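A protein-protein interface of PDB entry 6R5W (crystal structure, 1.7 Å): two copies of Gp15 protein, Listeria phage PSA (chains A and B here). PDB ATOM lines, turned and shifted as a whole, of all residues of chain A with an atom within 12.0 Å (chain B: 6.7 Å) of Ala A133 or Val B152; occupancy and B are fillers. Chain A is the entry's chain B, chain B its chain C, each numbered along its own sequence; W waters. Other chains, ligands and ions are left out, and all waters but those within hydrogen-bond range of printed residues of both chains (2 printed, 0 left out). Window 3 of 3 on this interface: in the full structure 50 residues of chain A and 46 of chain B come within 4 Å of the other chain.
O of Asn A135 lies close to N of Gln A128.
The backbone NH (N) of Gly A153 is in hydrogen-bond range of the backbone carbonyl oxygen (O) of Gln A136 (2.9 Å).
The side-chain hydroxyl (OG) of Ser A130 lies within hydrogen-bond range of the backbone NH (N) of Ala A132 (3.0 Å).
The backbone NH of Asn B138 is in hydrogen-bond range of the backbone carbonyl oxygen of Gly B151.
The side-chain amide nitrogen of Gln A128 is in hydrogen-bond range of the backbone carbonyl oxygen of Ser A154 (3.0 Å).
OG of Ser A130 lies within hydrogen-bond range of ND2 of Asn A135 (3.0 Å).
Hydrophobic or aromatic side chains of chain B that line the printed part of chain A: Val B150.
Hydrophobic or aromatic side chains of chain A within 4 Å of the printed part of chain B: Ala A127 and Ala A133.
Among the printed residues, pairs that only touch across the chains: Ala A127 with Asn B138 (3.2 Å), Ser A130 with Val B150 (3.7 Å), Thr A131 with Val B150 (3.7 Å), Thr A131 with Gly B151 (3.3 Å), Ala A133 with Gln B136 (3.4 Å), Ala A133 with Val B152 (3.5 Å) and Ala A133 with Gly B153 (3.6 Å).
Water W1 bridges O of Ser B134 (2.8 Å) and N of Ser A134 (3.4 Å).
Water W2 bridges O of Val B152 (2.8 Å) and N of Ala A133 (2.9 Å).
Asn A135 touches Asn B138, but with the chains exchanged Asn A138 does not touch Asn B135 (12.8 Å).
Gln A136 touches its own counterpart, Gln B136.
Gln A136 touches Ala B137, but with the chains exchanged Ala A137 does not touch Gln B136 (7.6 Å).
Gln A136 touches Asn B138, but with the chains exchanged Asn A138 does not touch Gln B136 (7.4 Å).
Of the 14 pairs that touch across the chains among the printed residues, 1 has its exchanged pair printed and touching as well.
O of Ser A130 is in hydrogen-bond range of ND2 of Asn B138 (3.0 Å).
The side-chain amide oxygen (OE1) of Gln B136 lies close to the side-chain amide oxygen (OE1) of Gln A136 (3.1 Å).
The side-chain amide nitrogen (ND2) of Asn B138 lies within hydrogen-bond range of the backbone carbonyl oxygen (O) of Gln A128 (3.5 Å).
The backbone carbonyl oxygen (O) of Asn A135 is in hydrogen-bond range of the side-chain amide nitrogen (ND2) of Asn B138, at 3.1 Å.
The side-chain amide nitrogen of Asn B138 sits at hydrogen-bond distance from the backbone carbonyl oxygen of Ala A132.
NE2 of Gln A136 lies within hydrogen-bond range of OD1 of Asn B138, at 2.8 Å.
The side-chain amide nitrogen (NE2) of Gln A136 is in hydrogen-bond range of the backbone carbonyl oxygen (O) of Ala B137.
Of the printed residues of chain B, Ser A130 touches Asn B138 (3.0 Å) and Val B150 (3.7 Å).
Of the printed residues of chain B, Thr A131 touches Val B150 and Gly B151.
Of the printed residues of chain B, Ala A133 touches Gln B136 (3.4 Å), Val B152 (3.5 Å) and Gly B153 (3.6 Å).
Of the printed residues of chain B, Asn A135 touches Asn B138.
Ala A137 touches none of the printed residues of chain B.
No residue of chain A comes within 4 Å of Gly B103.
No residue of chain A comes within 4 Å of Asn B135.
Of chain A, only Gln A136 comes within 4 Å of Ala B137.
Of the printed residues of chain A, Asn B138 touches Ala A127 (3.2 Å), Gln A128 (3.5 Å), Ser A130 (3.0 Å), Ala A132 (3.3 Å), Asn A135 (3.1 Å) and Gln A136 (2.8 Å).
No residue of chain A comes within 4 Å of Ile B149.
Of chain A, only Thr A131 comes within 4 Å of Gly B151.
Val B152 touches one residue of chain A.
No residue of chain A comes within 4 Å of Ser B154.
The nearest printed residue of chain B that does not touch Ala A133 is Asn B138 (4.003 Å).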
ATOM      1  N   SER A 125      29.719   4.266  -5.151  1.00  0.00           N
ATOM      2  CA  SER A 125      29.201   5.590  -4.865  1.00  0.00           C
ATOM      3  C   SER A 125      30.204   6.639  -5.332  1.00  0.00           C
ATOM      4  O   SER A 125      31.412   6.518  -5.079  1.00  0.00           O
ATOM      5  CB  SER A 125      28.925   5.764  -3.365  1.00  0.00           C
ATOM      6  OG  SER A 125      28.947   7.142  -3.107  1.00  0.00           O
ATOM      7  N   ALA A 126      29.721   7.642  -6.037  1.00  0.00           N
ATOM      8  CA  ALA A 126      30.586   8.676  -6.601  1.00  0.00           C
ATOM      9  C   ALA A 126      30.143  10.058  -6.162  1.00  0.00           C
ATOM     10  O   ALA A 126      28.935  10.339  -6.051  1.00  0.00           O
ATOM     11  CB  ALA A 126      30.597   8.592  -8.155  1.00  0.00           C
ATOM     12  N   ALA A 127      31.133  10.934  -5.984  1.00  0.00           N
ATOM     13  CA  ALA A 127      30.837  12.334  -5.733  1.00  0.00           C
ATOM     14  C   ALA A 127      30.450  13.046  -7.027  1.00  0.00           C
ATOM     15  O   ALA A 127      30.998  12.754  -8.066  1.00  0.00           O
ATOM     16  CB  ALA A 127      32.009  13.062  -5.130  1.00  0.00           C
ATOM     17  N   GLN A 128      29.518  14.010  -6.938  1.00  0.00           N
ATOM     18  CA  GLN A 128      29.358  14.998  -8.004  1.00  0.00           C
ATOM     19  C   GLN A 128      30.129  16.257  -7.638  1.00  0.00           C
ATOM     20  O   GLN A 128      30.578  16.441  -6.507  1.00  0.00           O
ATOM     21  CB  GLN A 128      27.868  15.344  -8.280  1.00  0.00           C
ATOM     22  CG  GLN A 128      27.045  14.138  -8.739  1.00  0.00           C
ATOM     23  CD  GLN A 128      25.689  14.546  -9.304  1.00  0.00           C
ATOM     24  OE1 GLN A 128      24.718  14.715  -8.560  1.00  0.00           O
ATOM     25  NE2 GLN A 128      25.632  14.701 -10.616  1.00  0.00           N
ATOM     26  N   GLN A 129      30.310  17.116  -8.649  1.00  0.00           N
ATOM     27  CA  GLN A 129      31.069  18.350  -8.553  1.00  0.00           C
ATOM     28  C   GLN A 129      30.184  19.452  -7.966  1.00  0.00           C
ATOM     29  O   GLN A 129      29.765  20.386  -8.654  1.00  0.00           O
ATOM     30  CB  GLN A 129      31.606  18.679  -9.936  1.00  0.00           C
ATOM     31  CG  GLN A 129      32.618  19.828  -9.983  1.00  0.00           C
ATOM     32  CD  GLN A 129      33.080  20.126 -11.386  1.00  0.00           C
ATOM     33  OE1 GLN A 129      33.316  19.215 -12.223  1.00  0.00           O
ATOM     34  NE2 GLN A 129      33.109  21.422 -11.697  1.00  0.00           N
ATOM     35  N   SER A 130      29.958  19.356  -6.659  1.00  0.00           N
ATOM     36  CA  SER A 130      28.951  20.209  -6.025  1.00  0.00           C
ATOM     37  C   SER A 130      29.170  20.337  -4.530  1.00  0.00           C
ATOM     38  O   SER A 130      29.558  19.370  -3.849  1.00  0.00           O
ATOM     39  CB  SER A 130      27.532  19.630  -6.345  1.00  0.00           C
ATOM     40  OG  SER A 130      26.514  20.264  -5.606  1.00  0.00           O
ATOM     41  N   THR A 131      28.846  21.542  -4.004  1.00  0.00           N
ATOM     42  CA  THR A 131      28.872  21.759  -2.557  1.00  0.00           C
ATOM     43  C   THR A 131      27.661  21.157  -1.864  1.00  0.00           C
ATOM     44  O   THR A 131      27.626  21.117  -0.639  1.00  0.00           O
ATOM     45  CB  THR A 131      28.925  23.261  -2.228  1.00  0.00           C
ATOM     46  OG1 THR A 131      27.804  23.870  -2.886  1.00  0.00           O
ATOM     47  CG2 THR A 131      30.223  23.877  -2.681  1.00  0.00           C
ATOM     48  N   ALA A 132      26.653  20.736  -2.602  1.00  0.00           N
ATOM     49  CA  ALA A 132      25.510  20.039  -2.020  1.00  0.00           C
ATOM     50  C   ALA A 132      25.834  18.550  -1.932  1.00  0.00           C
ATOM     51  O   ALA A 132      25.966  17.888  -2.968  1.00  0.00           O
ATOM     52  CB  ALA A 132      24.245  20.262  -2.856  1.00  0.00           C
ATOM     53  N   ALA A 133      25.890  18.017  -0.707  1.00  0.00           N
ATOM     54  CA  ALA A 133      26.228  16.619  -0.485  1.00  0.00           C
ATOM     55  C   ALA A 133      25.175  15.638  -0.963  1.00  0.00           C
ATOM     56  O   ALA A 133      25.470  14.440  -1.082  1.00  0.00           O
ATOM     57  CB  ALA A 133      26.495  16.401   1.000  1.00  0.00           C
ATOM     58  N   SER A 134      23.943  16.092  -1.249  1.00  0.00           N
ATOM     59  CA  SER A 134      22.968  15.238  -1.903  1.00  0.00           C
ATOM     60  C   SER A 134      23.287  15.031  -3.379  1.00  0.00           C
ATOM     61  O   SER A 134      22.694  14.162  -4.006  1.00  0.00           O
ATOM     62  CB  SER A 134      21.546  15.845  -1.733  1.00  0.00           C
ATOM     63  OG  SER A 134      21.604  17.207  -2.186  1.00  0.00           O
ATOM     64  N   ASN A 135      24.184  15.799  -3.942  1.00  0.00           N
ATOM     65  CA  ASN A 135      24.591  15.584  -5.336  1.00  0.00           C
ATOM     66  C   ASN A 135      25.762  14.580  -5.330  1.00  0.00           C
ATOM     67  O   ASN A 135      26.945  14.958  -5.297  1.00  0.00           O
ATOM     68  CB  ASN A 135      24.927  16.898  -5.979  1.00  0.00           C
ATOM     69  CG  ASN A 135      23.693  17.730  -6.273  1.00  0.00           C
ATOM     70  OD1 ASN A 135      22.580  17.198  -6.413  1.00  0.00           O
ATOM     71  ND2 ASN A 135      23.884  19.052  -6.334  1.00  0.00           N
ATOM     72  N   GLN A 136      25.398  13.307  -5.335  1.00  0.00           N
ATOM     73  CA  GLN A 136      26.286  12.181  -5.460  1.00  0.00           C
ATOM     74  C   GLN A 136      25.626  11.258  -6.479  1.00  0.00           C
ATOM     75  O   GLN A 136      24.508  11.518  -6.934  1.00  0.00           O
ATOM     76  CB  GLN A 136      26.530  11.510  -4.076  1.00  0.00           C
ATOM     77  CG  GLN A 136      27.112  12.501  -3.107  1.00  0.00           C
ATOM     78  CD  GLN A 136      27.751  11.891  -1.897  1.00  0.00           C
ATOM     79  OE1 GLN A 136      27.265  10.974  -1.332  1.00  0.00           O
ATOM     80  NE2 GLN A 136      28.916  12.419  -1.529  1.00  0.00           N
ATOM     81  N   ALA A 137      26.285  10.142  -6.800  1.00  0.00           N
ATOM     82  CA  ALA A 137      25.839   9.242  -7.874  1.00  0.00           C
ATOM     83  C   ALA A 137      26.032   7.799  -7.464  1.00  0.00           C
ATOM     84  O   ALA A 137      26.965   7.449  -6.735  1.00  0.00           O
ATOM     85  CB  ALA A 137      26.555   9.518  -9.200  1.00  0.00           C
ATOM     86  N   ASN A 138      25.135   6.951  -7.969  1.00  0.00           N
ATOM     87  CA  ASN A 138      25.294   5.508  -7.955  1.00  0.00           C
ATOM     88  C   ASN A 138      25.758   5.073  -9.354  1.00  0.00           C
ATOM     89  O   ASN A 138      25.112   5.419 -10.369  1.00  0.00           O
ATOM     90  CB  ASN A 138      24.009   4.776  -7.597  1.00  0.00           C
ATOM     91  CG  ASN A 138      23.702   4.837  -6.116  1.00  0.00           C
ATOM     92  OD1 ASN A 138      24.595   4.889  -5.283  1.00  0.00           O
ATOM     93  ND2 ASN A 138      22.420   4.803  -5.783  1.00  0.00           N
ATOM     94  N   GLY A 151      22.086   6.595 -11.278  1.00  0.00           N
ATOM     95  CA  GLY A 151      21.306   7.619 -10.572  1.00  0.00           C
ATOM     96  C   GLY A 151      22.165   8.755 -10.112  1.00  0.00           C
ATOM     97  O   GLY A 151      23.298   8.472  -9.692  1.00  0.00           O
ATOM     98  N   VAL A 152      21.686  10.001 -10.178  1.00  0.00           N
ATOM     99  CA  VAL A 152      22.445  11.150  -9.707  1.00  0.00           C
ATOM    100  C   VAL A 152      21.551  12.077  -8.868  1.00  0.00           C
ATOM    101  O   VAL A 152      20.333  12.102  -9.008  1.00  0.00           O
ATOM    102  CB  VAL A 152      23.053  11.979 -10.870  1.00  0.00           C
ATOM    103  CG1 VAL A 152      24.071  11.103 -11.657  1.00  0.00           C
ATOM    104  CG2 VAL A 152      21.914  12.521 -11.819  1.00  0.00           C
ATOM    105  N   GLY A 153      22.187  12.880  -8.020  1.00  0.00           N
ATOM    106  CA  GLY A 153      21.463  13.931  -7.324  1.00  0.00           C
ATOM    107  C   GLY A 153      20.967  15.022  -8.254  1.00  0.00           C
ATOM    108  O   GLY A 153      19.891  15.583  -8.037  1.00  0.00           O
ATOM    109  N   SER A 154      21.768  15.388  -9.260  1.00  0.00           N
ATOM    110  CA  SER A 154      21.367  16.393 -10.231  1.00  0.00           C
ATOM    111  C   SER A 154      21.991  16.099 -11.591  1.00  0.00           C
ATOM    112  O   SER A 154      23.231  16.041 -11.708  1.00  0.00           O
ATOM    113  CB  SER A 154      21.780  17.775  -9.757  1.00  0.00           C
ATOM    114  OG  SER A 154      21.709  18.671 -10.872  1.00  0.00           O
ATOM    115  N   VAL A 157      24.850  18.510 -12.911  1.00  0.00           N
ATOM    116  CA  VAL A 157      26.122  18.636 -12.224  1.00  0.00           C
ATOM    117  C   VAL A 157      27.048  17.524 -12.733  1.00  0.00           C
ATOM    118  O   VAL A 157      26.593  16.409 -12.988  1.00  0.00           O
ATOM    119  CB  VAL A 157      25.913  18.558 -10.702  1.00  0.00           C
ATOM    120  CG1 VAL A 157      27.262  18.611  -9.979  1.00  0.00           C
ATOM    121  CG2 VAL A 157      24.994  19.725 -10.285  1.00  0.00           C
ATOM    122  N   ASN A 158      28.332  17.841 -12.886  1.00  0.00           N
ATOM    123  CA  ASN A 158      29.301  16.838 -13.357  1.00  0.00           C
ATOM    124  C   ASN A 158      29.448  15.706 -12.299  1.00  0.00           C
ATOM    125  O   ASN A 158      29.187  15.873 -11.097  1.00  0.00           O
ATOM    126  CB  ASN A 158      30.642  17.499 -13.581  1.00  0.00           C
ATOM    127  CG  ASN A 158      30.664  18.524 -14.688  1.00  0.00           C
ATOM    128  OD1 ASN A 158      29.774  18.595 -15.514  1.00  0.00           O
ATOM    129  ND2 ASN A 158      31.699  19.345 -14.689  1.00  0.00           N
ATOM    130  N   THR A 159      29.884  14.540 -12.750  1.00  0.00           N
ATOM    131  CA  THR A 159      30.010  13.349 -11.917  1.00  0.00           C
ATOM    132  C   THR A 159      31.443  12.819 -11.992  1.00  0.00           C
ATOM    133  O   THR A 159      31.978  12.630 -13.087  1.00  0.00           O
ATOM    134  CB  THR A 159      28.995  12.285 -12.349  1.00  0.00           C
ATOM    135  OG1 THR A 159      27.660  12.811 -12.168  1.00  0.00           O
ATOM    136  CG2 THR A 159      29.114  10.974 -11.503  1.00  0.00           C
ATOM    137  N   GLY A 160      32.046  12.561 -10.836  1.00  0.00           N
ATOM    138  CA  GLY A 160      33.410  12.033 -10.821  1.00  0.00           C
ATOM    139  C   GLY A 160      33.487  10.521 -10.960  1.00  0.00           C
ATOM    140  O   GLY A 160      32.648   9.744 -10.490  1.00  0.00           O
ATOM    141  N   SER B 102      34.830  25.267  10.298  1.00  0.00           N
ATOM    142  CA  SER B 102      33.453  25.348   9.795  1.00  0.00           C
ATOM    143  C   SER B 102      32.846  24.010   9.405  1.00  0.00           C
ATOM    144  O   SER B 102      31.657  23.965   9.066  1.00  0.00           O
ATOM    145  CB  SER B 102      33.386  26.244   8.582  1.00  0.00           C
ATOM    146  OG  SER B 102      34.055  25.608   7.497  1.00  0.00           O
ATOM    147  N   GLY B 103      33.633  22.937   9.367  1.00  0.00           N
ATOM    148  CA  GLY B 103      33.166  21.673   8.873  1.00  0.00           C
ATOM    149  C   GLY B 103      33.378  21.448   7.398  1.00  0.00           C
ATOM    150  O   GLY B 103      33.188  20.329   6.940  1.00  0.00           O
ATOM    151  N   THR B 104      33.848  22.452   6.675  1.00  0.00           N
ATOM    152  CA  THR B 104      34.208  22.328   5.264  1.00  0.00           C
ATOM    153  C   THR B 104      35.550  23.027   5.049  1.00  0.00           C
ATOM    154  O   THR B 104      36.102  23.672   5.944  1.00  0.00           O
ATOM    155  CB  THR B 104      33.118  22.891   4.340  1.00  0.00           C
ATOM    156  OG1 THR B 104      32.982  24.300   4.574  1.00  0.00           O
ATOM    157  CG2 THR B 104      31.779  22.191   4.557  1.00  0.00           C
ATOM    158  N   GLN B 128      30.018   9.899   6.408  1.00  0.00           N
ATOM    159  CA  GLN B 128      30.086  10.565   7.708  1.00  0.00           C
ATOM    160  C   GLN B 128      29.699   9.574   8.804  1.00  0.00           C
ATOM    161  O   GLN B 128      29.200   8.485   8.547  1.00  0.00           O
ATOM    162  CB  GLN B 128      29.212  11.794   7.761  1.00  0.00           C
ATOM    163  CG  GLN B 128      29.614  12.859   6.798  1.00  0.00           C
ATOM    164  CD  GLN B 128      29.000  14.203   7.184  1.00  0.00           C
ATOM    165  OE1 GLN B 128      27.859  14.502   6.816  1.00  0.00           O
ATOM    166  NE2 GLN B 128      29.776  15.013   7.911  1.00  0.00           N
ATOM    167  N   SER B 134      22.083  10.407   4.335  1.00  0.00           N
ATOM    168  CA  SER B 134      22.239  11.728   3.755  1.00  0.00           C
ATOM    169  C   SER B 134      23.441  12.461   4.342  1.00  0.00           C
ATOM    170  O   SER B 134      23.856  13.487   3.814  1.00  0.00           O
ATOM    171  CB  SER B 134      20.970  12.572   3.961  1.00  0.00           C
ATOM    172  OG  SER B 134      20.672  12.613   5.345  1.00  0.00           O
ATOM    173  N   ASN B 135      23.986  11.986   5.452  1.00  0.00           N
ATOM    174  CA  ASN B 135      25.232  12.532   6.030  1.00  0.00           C
ATOM    175  C   ASN B 135      26.419  11.792   5.383  1.00  0.00           C
ATOM    176  O   ASN B 135      26.912  10.754   5.865  1.00  0.00           O
ATOM    177  CB  ASN B 135      25.226  12.380   7.536  1.00  0.00           C
ATOM    178  CG  ASN B 135      24.280  13.408   8.183  1.00  0.00           C
ATOM    179  OD1 ASN B 135      23.991  14.461   7.556  1.00  0.00           O
ATOM    180  ND2 ASN B 135      23.818  13.136   9.391  1.00  0.00           N
ATOM    181  N   GLN B 136      26.773  12.302   4.199  1.00  0.00           N
ATOM    182  CA  GLN B 136      27.957  11.935   3.435  1.00  0.00           C
ATOM    183  C   GLN B 136      28.608  13.233   2.947  1.00  0.00           C
ATOM    184  O   GLN B 136      28.102  14.359   3.176  1.00  0.00           O
ATOM    185  CB  GLN B 136      27.568  10.987   2.285  1.00  0.00           C
ATOM    186  CG  GLN B 136      26.911   9.732   2.813  1.00  0.00           C
ATOM    187  CD  GLN B 136      26.779   8.611   1.847  1.00  0.00           C
ATOM    188  OE1 GLN B 136      26.389   8.818   0.714  1.00  0.00           O
ATOM    189  NE2 GLN B 136      27.135   7.446   2.261  1.00  0.00           N
ATOM    190  N   ALA B 137      29.752  13.099   2.236  1.00  0.00           N
ATOM    191  CA  ALA B 137      30.547  14.277   1.935  1.00  0.00           C
ATOM    192  C   ALA B 137      31.036  14.139   0.505  1.00  0.00           C
ATOM    193  O   ALA B 137      31.284  13.045   0.045  1.00  0.00           O
ATOM    194  CB  ALA B 137      31.724  14.436   2.904  1.00  0.00           C
ATOM    195  N   ASN B 138      31.124  15.267  -0.180  1.00  0.00           N
ATOM    196  CA  ASN B 138      31.843  15.409  -1.432  1.00  0.00           C
ATOM    197  C   ASN B 138      33.197  16.011  -1.115  1.00  0.00           C
ATOM    198  O   ASN B 138      33.280  17.082  -0.499  1.00  0.00           O
ATOM    199  CB  ASN B 138      31.120  16.300  -2.433  1.00  0.00           C
ATOM    200  CG  ASN B 138      29.943  15.645  -3.039  1.00  0.00           C
ATOM    201  OD1 ASN B 138      29.884  14.420  -3.210  1.00  0.00           O
ATOM    202  ND2 ASN B 138      28.946  16.483  -3.420  1.00  0.00           N
ATOM    203  N   ILE B 149      37.069  19.255   1.920  1.00  0.00           N
ATOM    204  CA  ILE B 149      35.698  18.813   2.165  1.00  0.00           C
ATOM    205  C   ILE B 149      34.803  19.929   1.626  1.00  0.00           C
ATOM    206  O   ILE B 149      34.672  20.989   2.247  1.00  0.00           O
ATOM    207  CB  ILE B 149      35.459  18.517   3.640  1.00  0.00           C
ATOM    208  CG1 ILE B 149      36.350  17.329   4.051  1.00  0.00           C
ATOM    209  CG2 ILE B 149      33.983  18.187   3.905  1.00  0.00           C
ATOM    210  CD1 ILE B 149      36.412  17.120   5.519  1.00  0.00           C
ATOM    211  N   VAL B 150      34.214  19.718   0.449  1.00  0.00           N
ATOM    212  CA  VAL B 150      33.499  20.818  -0.191  1.00  0.00           C
ATOM    213  C   VAL B 150      32.022  20.841   0.199  1.00  0.00           C
ATOM    214  O   VAL B 150      31.408  21.913   0.192  1.00  0.00           O
ATOM    215  CB  VAL B 150      33.668  20.821  -1.723  1.00  0.00           C
ATOM    216  CG1 VAL B 150      35.152  20.850  -2.082  1.00  0.00           C
ATOM    217  CG2 VAL B 150      32.915  19.725  -2.343  1.00  0.00           C
ATOM    218  N   GLY B 151      31.426  19.703   0.485  1.00  0.00           N
ATOM    219  CA  GLY B 151      30.052  19.621   0.948  1.00  0.00           C
ATOM    220  C   GLY B 151      29.842  18.457   1.884  1.00  0.00           C
ATOM    221  O   GLY B 151      30.459  17.392   1.699  1.00  0.00           O
ATOM    222  N   VAL B 152      29.025  18.653   2.932  1.00  0.00           N
ATOM    223  CA  VAL B 152      28.724  17.587   3.882  1.00  0.00           C
ATOM    224  C   VAL B 152      27.231  17.638   4.190  1.00  0.00           C
ATOM    225  O   VAL B 152      26.593  18.691   4.061  1.00  0.00           O
ATOM    226  CB  VAL B 152      29.523  17.677   5.219  1.00  0.00           C
ATOM    227  CG1 VAL B 152      31.006  17.539   5.038  1.00  0.00           C
ATOM    228  CG2 VAL B 152      29.181  19.038   5.948  1.00  0.00           C
ATOM    229  N   GLY B 153      26.680  16.503   4.579  1.00  0.00           N
ATOM    230  CA  GLY B 153      25.305  16.493   5.030  1.00  0.00           C
ATOM    231  C   GLY B 153      25.142  17.247   6.331  1.00  0.00           C
ATOM    232  O   GLY B 153      24.180  17.987   6.510  1.00  0.00           O
ATOM    233  N   SER B 154      26.116  17.118   7.230  1.00  0.00           N
ATOM    234  CA  SER B 154      26.065  17.867   8.473  1.00  0.00           C
ATOM    235  C   SER B 154      27.471  18.280   8.887  1.00  0.00           C
ATOM    236  O   SER B 154      28.330  17.408   9.102  1.00  0.00           O
ATOM    237  CB  SER B 154      25.414  17.030   9.555  1.00  0.00           C
ATOM    238  OG  SER B 154      25.677  17.677  10.807  1.00  0.00           O
ATOM    239  N   VAL B 155      27.684  19.594   9.079  1.00  0.00           N
ATOM    240  CA  VAL B 155      28.995  20.057   9.511  1.00  0.00           C
ATOM    241  C   VAL B 155      29.342  19.620  10.921  1.00  0.00           C
ATOM    242  O   VAL B 155      30.546  19.616  11.296  1.00  0.00           O
ATOM    243  CB  VAL B 155      29.108  21.592   9.414  1.00  0.00           C
ATOM    244  CG1 VAL B 155      28.851  22.054   7.991  1.00  0.00           C
ATOM    245  CG2 VAL B 155      28.131  22.269  10.392  1.00  0.00           C
ATOM    246  N   ASP B 156      28.365  19.156  11.694  1.00  0.00           N
ATOM    247  CA  ASP B 156      28.630  18.760  13.067  1.00  0.00           C
ATOM    248  C   ASP B 156      28.839  17.277  13.242  1.00  0.00           C
ATOM    249  O   ASP B 156      28.774  16.791  14.368  1.00  0.00           O
ATOM    250  CB  ASP B 156      27.482  19.253  13.982  1.00  0.00           C
ATOM    251  CG  ASP B 156      27.376  20.765  13.988  1.00  0.00           C
ATOM    252  OD1 ASP B 156      28.425  21.430  14.168  1.00  0.00           O
ATOM    253  OD2 ASP B 156      26.266  21.282  13.741  1.00  0.00           O
ATOM    254  N   VAL B 157      29.038  16.519  12.156  1.00  0.00           N
ATOM    255  CA  VAL B 157      29.310  15.092  12.221  1.00  0.00           C
ATOM    256  C   VAL B 157      30.674  14.850  11.567  1.00  0.00           C
ATOM    257  O   VAL B 157      31.007  15.519  10.592  1.00  0.00           O
ATOM    258  CB  VAL B 157      28.206  14.305  11.481  1.00  0.00           C
ATOM    259  CG1 VAL B 157      28.539  12.799  11.483  1.00  0.00           C
ATOM    260  CG2 VAL B 157      26.824  14.526  12.194  1.00  0.00           C
ATOM    261  N   THR B 159      33.774  13.167   9.440  1.00  0.00           N
ATOM    262  CA  THR B 159      33.854  12.700   8.039  1.00  0.00           C
ATOM    263  C   THR B 159      35.042  11.750   7.874  1.00  0.00           C
ATOM    264  O   THR B 159      36.147  12.037   8.346  1.00  0.00           O
ATOM    265  CB  THR B 159      33.982  13.925   7.115  1.00  0.00           C
ATOM    266  OG1 THR B 159      32.795  14.757   7.180  1.00  0.00           O
ATOM    267  CG2 THR B 159      34.183  13.483   5.649  1.00  0.00           C
HETATM  268  O   HOH W   1      22.766  14.788   1.650  1.00  0.00           O
HETATM  269  O   HOH W   2      25.339  19.580   1.690  1.00  0.00           O
